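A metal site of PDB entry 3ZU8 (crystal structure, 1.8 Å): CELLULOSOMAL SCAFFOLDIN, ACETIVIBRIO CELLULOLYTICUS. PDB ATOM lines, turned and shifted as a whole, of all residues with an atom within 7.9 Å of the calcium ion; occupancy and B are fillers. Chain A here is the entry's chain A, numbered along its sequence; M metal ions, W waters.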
ATOM      1  N   ALA A  17      20.722   3.827 -24.549  1.00  0.00           N
ATOM      2  CA  ALA A  17      19.843   2.720 -24.134  1.00  0.00           C
ATOM      3  C   ALA A  17      18.664   3.250 -23.315  1.00  0.00           C
ATOM      4  O   ALA A  17      17.503   2.991 -23.635  1.00  0.00           O
ATOM      5  CB  ALA A  17      20.624   1.688 -23.341  1.00  0.00           C
ATOM      6  N   ILE A  22      12.776   8.404 -28.838  1.00  0.00           N
ATOM      7  CA  ILE A  22      13.307   7.526 -29.887  1.00  0.00           C
ATOM      8  C   ILE A  22      13.334   8.356 -31.173  1.00  0.00           C
ATOM      9  O   ILE A  22      12.442   9.159 -31.415  1.00  0.00           O
ATOM     10  CB  ILE A  22      12.494   6.225 -30.000  1.00  0.00           C
ATOM     11  CG1 ILE A  22      12.625   5.431 -28.682  1.00  0.00           C
ATOM     12  CG2 ILE A  22      12.935   5.392 -31.200  1.00  0.00           C
ATOM     13  CD1 ILE A  22      11.711   4.218 -28.578  1.00  0.00           C
ATOM     14  N   TYR A  46       9.196  -0.863 -34.734  1.00  0.00           N
ATOM     15  CA  TYR A  46       8.712  -1.785 -33.688  1.00  0.00           C
ATOM     16  C   TYR A  46       9.575  -1.713 -32.438  1.00  0.00           C
ATOM     17  O   TYR A  46      10.799  -1.655 -32.538  1.00  0.00           O
ATOM     18  CB  TYR A  46       8.749  -3.222 -34.205  1.00  0.00           C
ATOM     19  CG  TYR A  46       7.834  -3.468 -35.373  1.00  0.00           C
ATOM     20  CD1 TYR A  46       6.489  -3.774 -35.180  1.00  0.00           C
ATOM     21  CD2 TYR A  46       8.319  -3.382 -36.686  1.00  0.00           C
ATOM     22  CE1 TYR A  46       5.647  -4.007 -36.256  1.00  0.00           C
ATOM     23  CE2 TYR A  46       7.463  -3.613 -37.771  1.00  0.00           C
ATOM     24  CZ  TYR A  46       6.149  -3.917 -37.540  1.00  0.00           C
ATOM     25  OH  TYR A  46       5.299  -4.151 -38.604  1.00  0.00           O
ATOM     26  N   PHE A  47       8.929  -1.741 -31.271  1.00  0.00           N
ATOM     27  CA  PHE A  47       9.662  -1.535 -30.014  1.00  0.00           C
ATOM     28  C   PHE A  47       8.877  -2.085 -28.825  1.00  0.00           C
ATOM     29  O   PHE A  47       7.707  -2.426 -28.960  1.00  0.00           O
ATOM     30  CB  PHE A  47       9.929  -0.037 -29.819  1.00  0.00           C
ATOM     31  CG  PHE A  47       8.681   0.824 -29.665  1.00  0.00           C
ATOM     32  CD1 PHE A  47       7.963   1.249 -30.783  1.00  0.00           C
ATOM     33  CD2 PHE A  47       8.263   1.254 -28.406  1.00  0.00           C
ATOM     34  CE1 PHE A  47       6.813   2.050 -30.644  1.00  0.00           C
ATOM     35  CE2 PHE A  47       7.129   2.056 -28.248  1.00  0.00           C
ATOM     36  CZ  PHE A  47       6.417   2.459 -29.370  1.00  0.00           C
ATOM     37  N   THR A  48       9.536  -2.200 -27.670  1.00  0.00           N
ATOM     38  CA  THR A  48       8.833  -2.450 -26.426  1.00  0.00           C
ATOM     39  C   THR A  48       8.739  -1.119 -25.689  1.00  0.00           C
ATOM     40  O   THR A  48       9.746  -0.405 -25.566  1.00  0.00           O
ATOM     41  CB  THR A  48       9.507  -3.542 -25.538  1.00  0.00           C
ATOM     42  OG1 THR A  48      10.825  -3.135 -25.147  1.00  0.00           O
ATOM     43  CG2 THR A  48       9.630  -4.855 -26.304  1.00  0.00           C
ATOM     44  N   VAL A  49       7.536  -0.764 -25.246  1.00  0.00           N
ATOM     45  CA  VAL A  49       7.267   0.568 -24.720  1.00  0.00           C
ATOM     46  C   VAL A  49       7.926   0.855 -23.363  1.00  0.00           C
ATOM     47  O   VAL A  49       8.237   2.004 -23.065  1.00  0.00           O
ATOM     48  CB  VAL A  49       5.755   0.880 -24.688  1.00  0.00           C
ATOM     49  CG1 VAL A  49       5.039   0.003 -23.658  1.00  0.00           C
ATOM     50  CG2 VAL A  49       5.504   2.373 -24.404  1.00  0.00           C
ATOM     51  N   ASP A  50       8.139  -0.189 -22.558  1.00  0.00           N
ATOM     52  CA  ASP A  50       8.777  -0.068 -21.242  1.00  0.00           C
ATOM     53  C   ASP A  50       8.021   0.895 -20.338  1.00  0.00           C
ATOM     54  O   ASP A  50       8.581   1.862 -19.825  1.00  0.00           O
ATOM     55  CB  ASP A  50      10.235   0.388 -21.359  1.00  0.00           C
ATOM     56  CG  ASP A  50      11.101  -0.665 -22.016  1.00  0.00           C
ATOM     57  OD1 ASP A  50      11.105  -1.811 -21.543  1.00  0.00           O
ATOM     58  OD2 ASP A  50      11.778  -0.330 -23.009  1.00  0.00           O
ATOM     59  N   GLY A  51       6.736   0.605 -20.147  1.00  0.00           N
ATOM     60  CA  GLY A  51       5.852   1.496 -19.426  1.00  0.00           C
ATOM     61  C   GLY A  51       4.990   2.248 -20.417  1.00  0.00           C
ATOM     62  O   GLY A  51       5.393   3.270 -20.966  1.00  0.00           O
ATOM     63  N   GLY A  82      10.945  -8.194 -28.596  1.00  0.00           N
ATOM     64  CA  GLY A  82      11.364  -6.883 -29.058  1.00  0.00           C
ATOM     65  C   GLY A  82      10.248  -5.971 -29.528  1.00  0.00           C
ATOM     66  O   GLY A  82      10.500  -4.851 -29.994  1.00  0.00           O
ATOM     67  N   ALA A  83       9.011  -6.425 -29.408  1.00  0.00           N
ATOM     68  CA  ALA A  83       7.914  -5.658 -29.993  1.00  0.00           C
ATOM     69  C   ALA A  83       6.590  -5.837 -29.251  1.00  0.00           C
ATOM     70  O   ALA A  83       5.904  -6.839 -29.442  1.00  0.00           O
ATOM     71  CB  ALA A  83       7.751  -6.015 -31.465  1.00  0.00           C
ATOM     72  N   ASP A  84       6.223  -4.851 -28.436  1.00  0.00           N
ATOM     73  CA  ASP A  84       4.857  -4.830 -27.941  1.00  0.00           C
ATOM     74  C   ASP A  84       4.036  -3.692 -28.551  1.00  0.00           C
ATOM     75  O   ASP A  84       2.835  -3.632 -28.343  1.00  0.00           O
ATOM     76  CB  ASP A  84       4.756  -4.887 -26.413  1.00  0.00           C
ATOM     77  CG  ASP A  84       5.479  -3.742 -25.722  1.00  0.00           C
ATOM     78  OD1 ASP A  84       5.612  -2.653 -26.311  1.00  0.00           O
ATOM     79  OD2 ASP A  84       5.918  -3.949 -24.574  1.00  0.00           O
ATOM     80  N   LYS A 112       6.947   9.816 -24.653  1.00  0.00           N
ATOM     81  CA  LYS A 112       5.768   9.597 -23.843  1.00  0.00           C
ATOM     82  C   LYS A 112       5.267  10.920 -23.284  1.00  0.00           C
ATOM     83  O   LYS A 112       6.016  11.868 -23.148  1.00  0.00           O
ATOM     84  CB  LYS A 112       6.114   8.674 -22.670  1.00  0.00           C
ATOM     85  CG  LYS A 112       6.651   7.328 -23.163  1.00  0.00           C
ATOM     86  CD  LYS A 112       7.053   6.450 -21.959  1.00  0.00           C
ATOM     87  CE  LYS A 112       7.752   5.188 -22.467  1.00  0.00           C
ATOM     88  NZ  LYS A 112       8.048   4.196 -21.382  1.00  0.00           N
ATOM     89  N   ASN A 117      11.246   7.275 -19.342  1.00  0.00           N
ATOM     90  CA  ASN A 117      12.191   6.599 -20.222  1.00  0.00           C
ATOM     91  C   ASN A 117      11.695   5.373 -20.979  1.00  0.00           C
ATOM     92  O   ASN A 117      10.818   4.633 -20.500  1.00  0.00           O
ATOM     93  CB  ASN A 117      13.445   6.204 -19.435  1.00  0.00           C
ATOM     94  CG  ASN A 117      14.315   7.399 -19.085  1.00  0.00           C
ATOM     95  OD1 ASN A 117      14.265   8.430 -19.749  1.00  0.00           O
ATOM     96  ND2 ASN A 117      15.123   7.259 -18.037  1.00  0.00           N
ATOM     97  N   TYR A 118      12.293   5.183 -22.157  1.00  0.00           N
ATOM     98  CA  TYR A 118      12.311   3.911 -22.881  1.00  0.00           C
ATOM     99  C   TYR A 118      13.619   3.180 -22.587  1.00  0.00           C
ATOM    100  O   TYR A 118      14.607   3.807 -22.191  1.00  0.00           O
ATOM    101  CB  TYR A 118      12.292   4.165 -24.393  1.00  0.00           C
ATOM    102  CG  TYR A 118      11.071   4.851 -24.937  1.00  0.00           C
ATOM    103  CD1 TYR A 118       9.930   4.125 -25.262  1.00  0.00           C
ATOM    104  CD2 TYR A 118      11.076   6.230 -25.178  1.00  0.00           C
ATOM    105  CE1 TYR A 118       8.819   4.764 -25.794  1.00  0.00           C
ATOM    106  CE2 TYR A 118       9.957   6.865 -25.708  1.00  0.00           C
ATOM    107  CZ  TYR A 118       8.834   6.128 -26.021  1.00  0.00           C
ATOM    108  OH  TYR A 118       7.734   6.773 -26.547  1.00  0.00           O
ATOM    109  N   ASN A 119      13.638   1.867 -22.802  1.00  0.00           N
ATOM    110  CA  ASN A 119      14.890   1.132 -22.954  1.00  0.00           C
ATOM    111  C   ASN A 119      15.019   0.742 -24.422  1.00  0.00           C
ATOM    112  O   ASN A 119      14.327  -0.156 -24.866  1.00  0.00           O
ATOM    113  CB  ASN A 119      14.882  -0.143 -22.123  1.00  0.00           C
ATOM    114  CG  ASN A 119      16.052  -1.065 -22.459  1.00  0.00           C
ATOM    115  OD1 ASN A 119      17.110  -0.599 -22.876  1.00  0.00           O
ATOM    116  ND2 ASN A 119      15.863  -2.370 -22.260  1.00  0.00           N
ATOM    117  N   GLN A 120      15.888   1.386 -25.176  1.00  0.00           N
ATOM    118  CA  GLN A 120      15.952   1.121 -26.611  1.00  0.00           C
ATOM    119  C   GLN A 120      16.608  -0.217 -26.931  1.00  0.00           C
ATOM    120  O   GLN A 120      16.373  -0.799 -27.996  1.00  0.00           O
ATOM    121  CB  GLN A 120      16.753   2.207 -27.326  1.00  0.00           C
ATOM    122  CG  GLN A 120      16.260   3.628 -27.105  1.00  0.00           C
ATOM    123  CD  GLN A 120      16.620   4.508 -28.270  1.00  0.00           C
ATOM    124  OE1 GLN A 120      15.981   4.423 -29.312  1.00  0.00           O
ATOM    125  NE2 GLN A 120      17.656   5.336 -28.111  1.00  0.00           N
ATOM    126  N   ALA A 121      17.427  -0.710 -26.006  1.00  0.00           N
ATOM    127  CA  ALA A 121      18.302  -1.859 -26.297  1.00  0.00           C
ATOM    128  C   ALA A 121      17.559  -3.114 -26.760  1.00  0.00           C
ATOM    129  O   ALA A 121      18.077  -3.873 -27.581  1.00  0.00           O
ATOM    130  CB  ALA A 121      19.198  -2.180 -25.097  1.00  0.00           C
ATOM    131  N   ASP A 122      16.356  -3.334 -26.222  1.00  0.00           N
ATOM    132  CA  ASP A 122      15.569  -4.530 -26.550  1.00  0.00           C
ATOM    133  C   ASP A 122      14.573  -4.325 -27.712  1.00  0.00           C
ATOM    134  O   ASP A 122      13.810  -5.230 -28.007  1.00  0.00           O
ATOM    135  CB  ASP A 122      14.835  -5.069 -25.318  1.00  0.00           C
ATOM    136  CG  ASP A 122      13.663  -4.192 -24.883  1.00  0.00           C
ATOM    137  OD1 ASP A 122      13.724  -2.979 -25.121  1.00  0.00           O
ATOM    138  OD2 ASP A 122      12.672  -4.701 -24.313  1.00  0.00           O
ATOM    139  N   ASP A 123      14.607  -3.159 -28.354  1.00  0.00           N
ATOM    140  CA  ASP A 123      13.610  -2.844 -29.391  1.00  0.00           C
ATOM    141  C   ASP A 123      13.941  -3.532 -30.707  1.00  0.00           C
ATOM    142  O   ASP A 123      15.049  -3.418 -31.221  1.00  0.00           O
ATOM    143  CB  ASP A 123      13.511  -1.328 -29.609  1.00  0.00           C
ATOM    144  CG  ASP A 123      12.932  -0.590 -28.404  1.00  0.00           C
ATOM    145  OD1 ASP A 123      12.282  -1.260 -27.574  1.00  0.00           O
ATOM    146  OD2 ASP A 123      13.093   0.639 -28.312  1.00  0.00           O
ATOM    147  N   TYR A 124      12.937  -4.219 -31.261  1.00  0.00           N
ATOM    148  CA  TYR A 124      13.077  -4.928 -32.535  1.00  0.00           C
ATOM    149  C   TYR A 124      13.754  -4.093 -33.610  1.00  0.00           C
ATOM    150  O   TYR A 124      14.686  -4.556 -34.249  1.00  0.00           O
ATOM    151  CB  TYR A 124      11.685  -5.345 -33.009  1.00  0.00           C
ATOM    152  CG  TYR A 124      11.646  -6.162 -34.290  1.00  0.00           C
ATOM    153  CD1 TYR A 124      11.737  -7.544 -34.239  1.00  0.00           C
ATOM    154  CD2 TYR A 124      11.464  -5.554 -35.533  1.00  0.00           C
ATOM    155  CE1 TYR A 124      11.662  -8.317 -35.413  1.00  0.00           C
ATOM    156  CE2 TYR A 124      11.407  -6.319 -36.711  1.00  0.00           C
ATOM    157  CZ  TYR A 124      11.502  -7.692 -36.632  1.00  0.00           C
ATOM    158  OH  TYR A 124      11.448  -8.470 -37.776  1.00  0.00           O
ATOM    159  N   PHE A 126      15.445  -1.210 -33.332  1.00  0.00           N
ATOM    160  CA  PHE A 126      16.540  -0.350 -32.885  1.00  0.00           C
ATOM    161  C   PHE A 126      17.869  -0.832 -33.432  1.00  0.00           C
ATOM    162  O   PHE A 126      18.210  -2.005 -33.331  1.00  0.00           O
ATOM    163  CB  PHE A 126      16.614  -0.314 -31.355  1.00  0.00           C
ATOM    164  CG  PHE A 126      17.726   0.549 -30.795  1.00  0.00           C
ATOM    165  CD1 PHE A 126      17.750   1.917 -31.024  1.00  0.00           C
ATOM    166  CD2 PHE A 126      18.718  -0.008 -29.988  1.00  0.00           C
ATOM    167  CE1 PHE A 126      18.771   2.740 -30.451  1.00  0.00           C
ATOM    168  CE2 PHE A 126      19.731   0.798 -29.429  1.00  0.00           C
ATOM    169  CZ  PHE A 126      19.753   2.159 -29.677  1.00  0.00           C
HETATM  170 CA    CA M   1      12.153  -1.089 -25.184  1.00  0.00          CA
HETATM  171  O   HOH W   1      11.903   1.319 -26.030  1.00  0.00           O
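The backbone carbonyl oxygen (O) of Asp 50 lies within hydrogen-bond range of the side-chain amino group (NZ) of Lys 112 (2.9 Å). The side-chain amide oxygen of Asn 119 sits at hydrogen-bond distance from the backbone NH of Ala 121, 3.1 Å away.
Within 4 Å of the calcium ion: Thr 48, Asp 50, Asn 119, Asp 122 and Asp 123.
The calcium ion is bound by OD2 of Asp 50 (2.3 Å), O of Asn 119 (2.4 Å), OD1 of Asp 123 (2.4 Å), OG1 of Thr 48 (2.4 Å), OD1 of Asp 122 (2.5 Å), O of Thr 48 (2.5 Å) and water W1 (2.6 Å). The calcium ion has seven donor atoms within binding distance.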
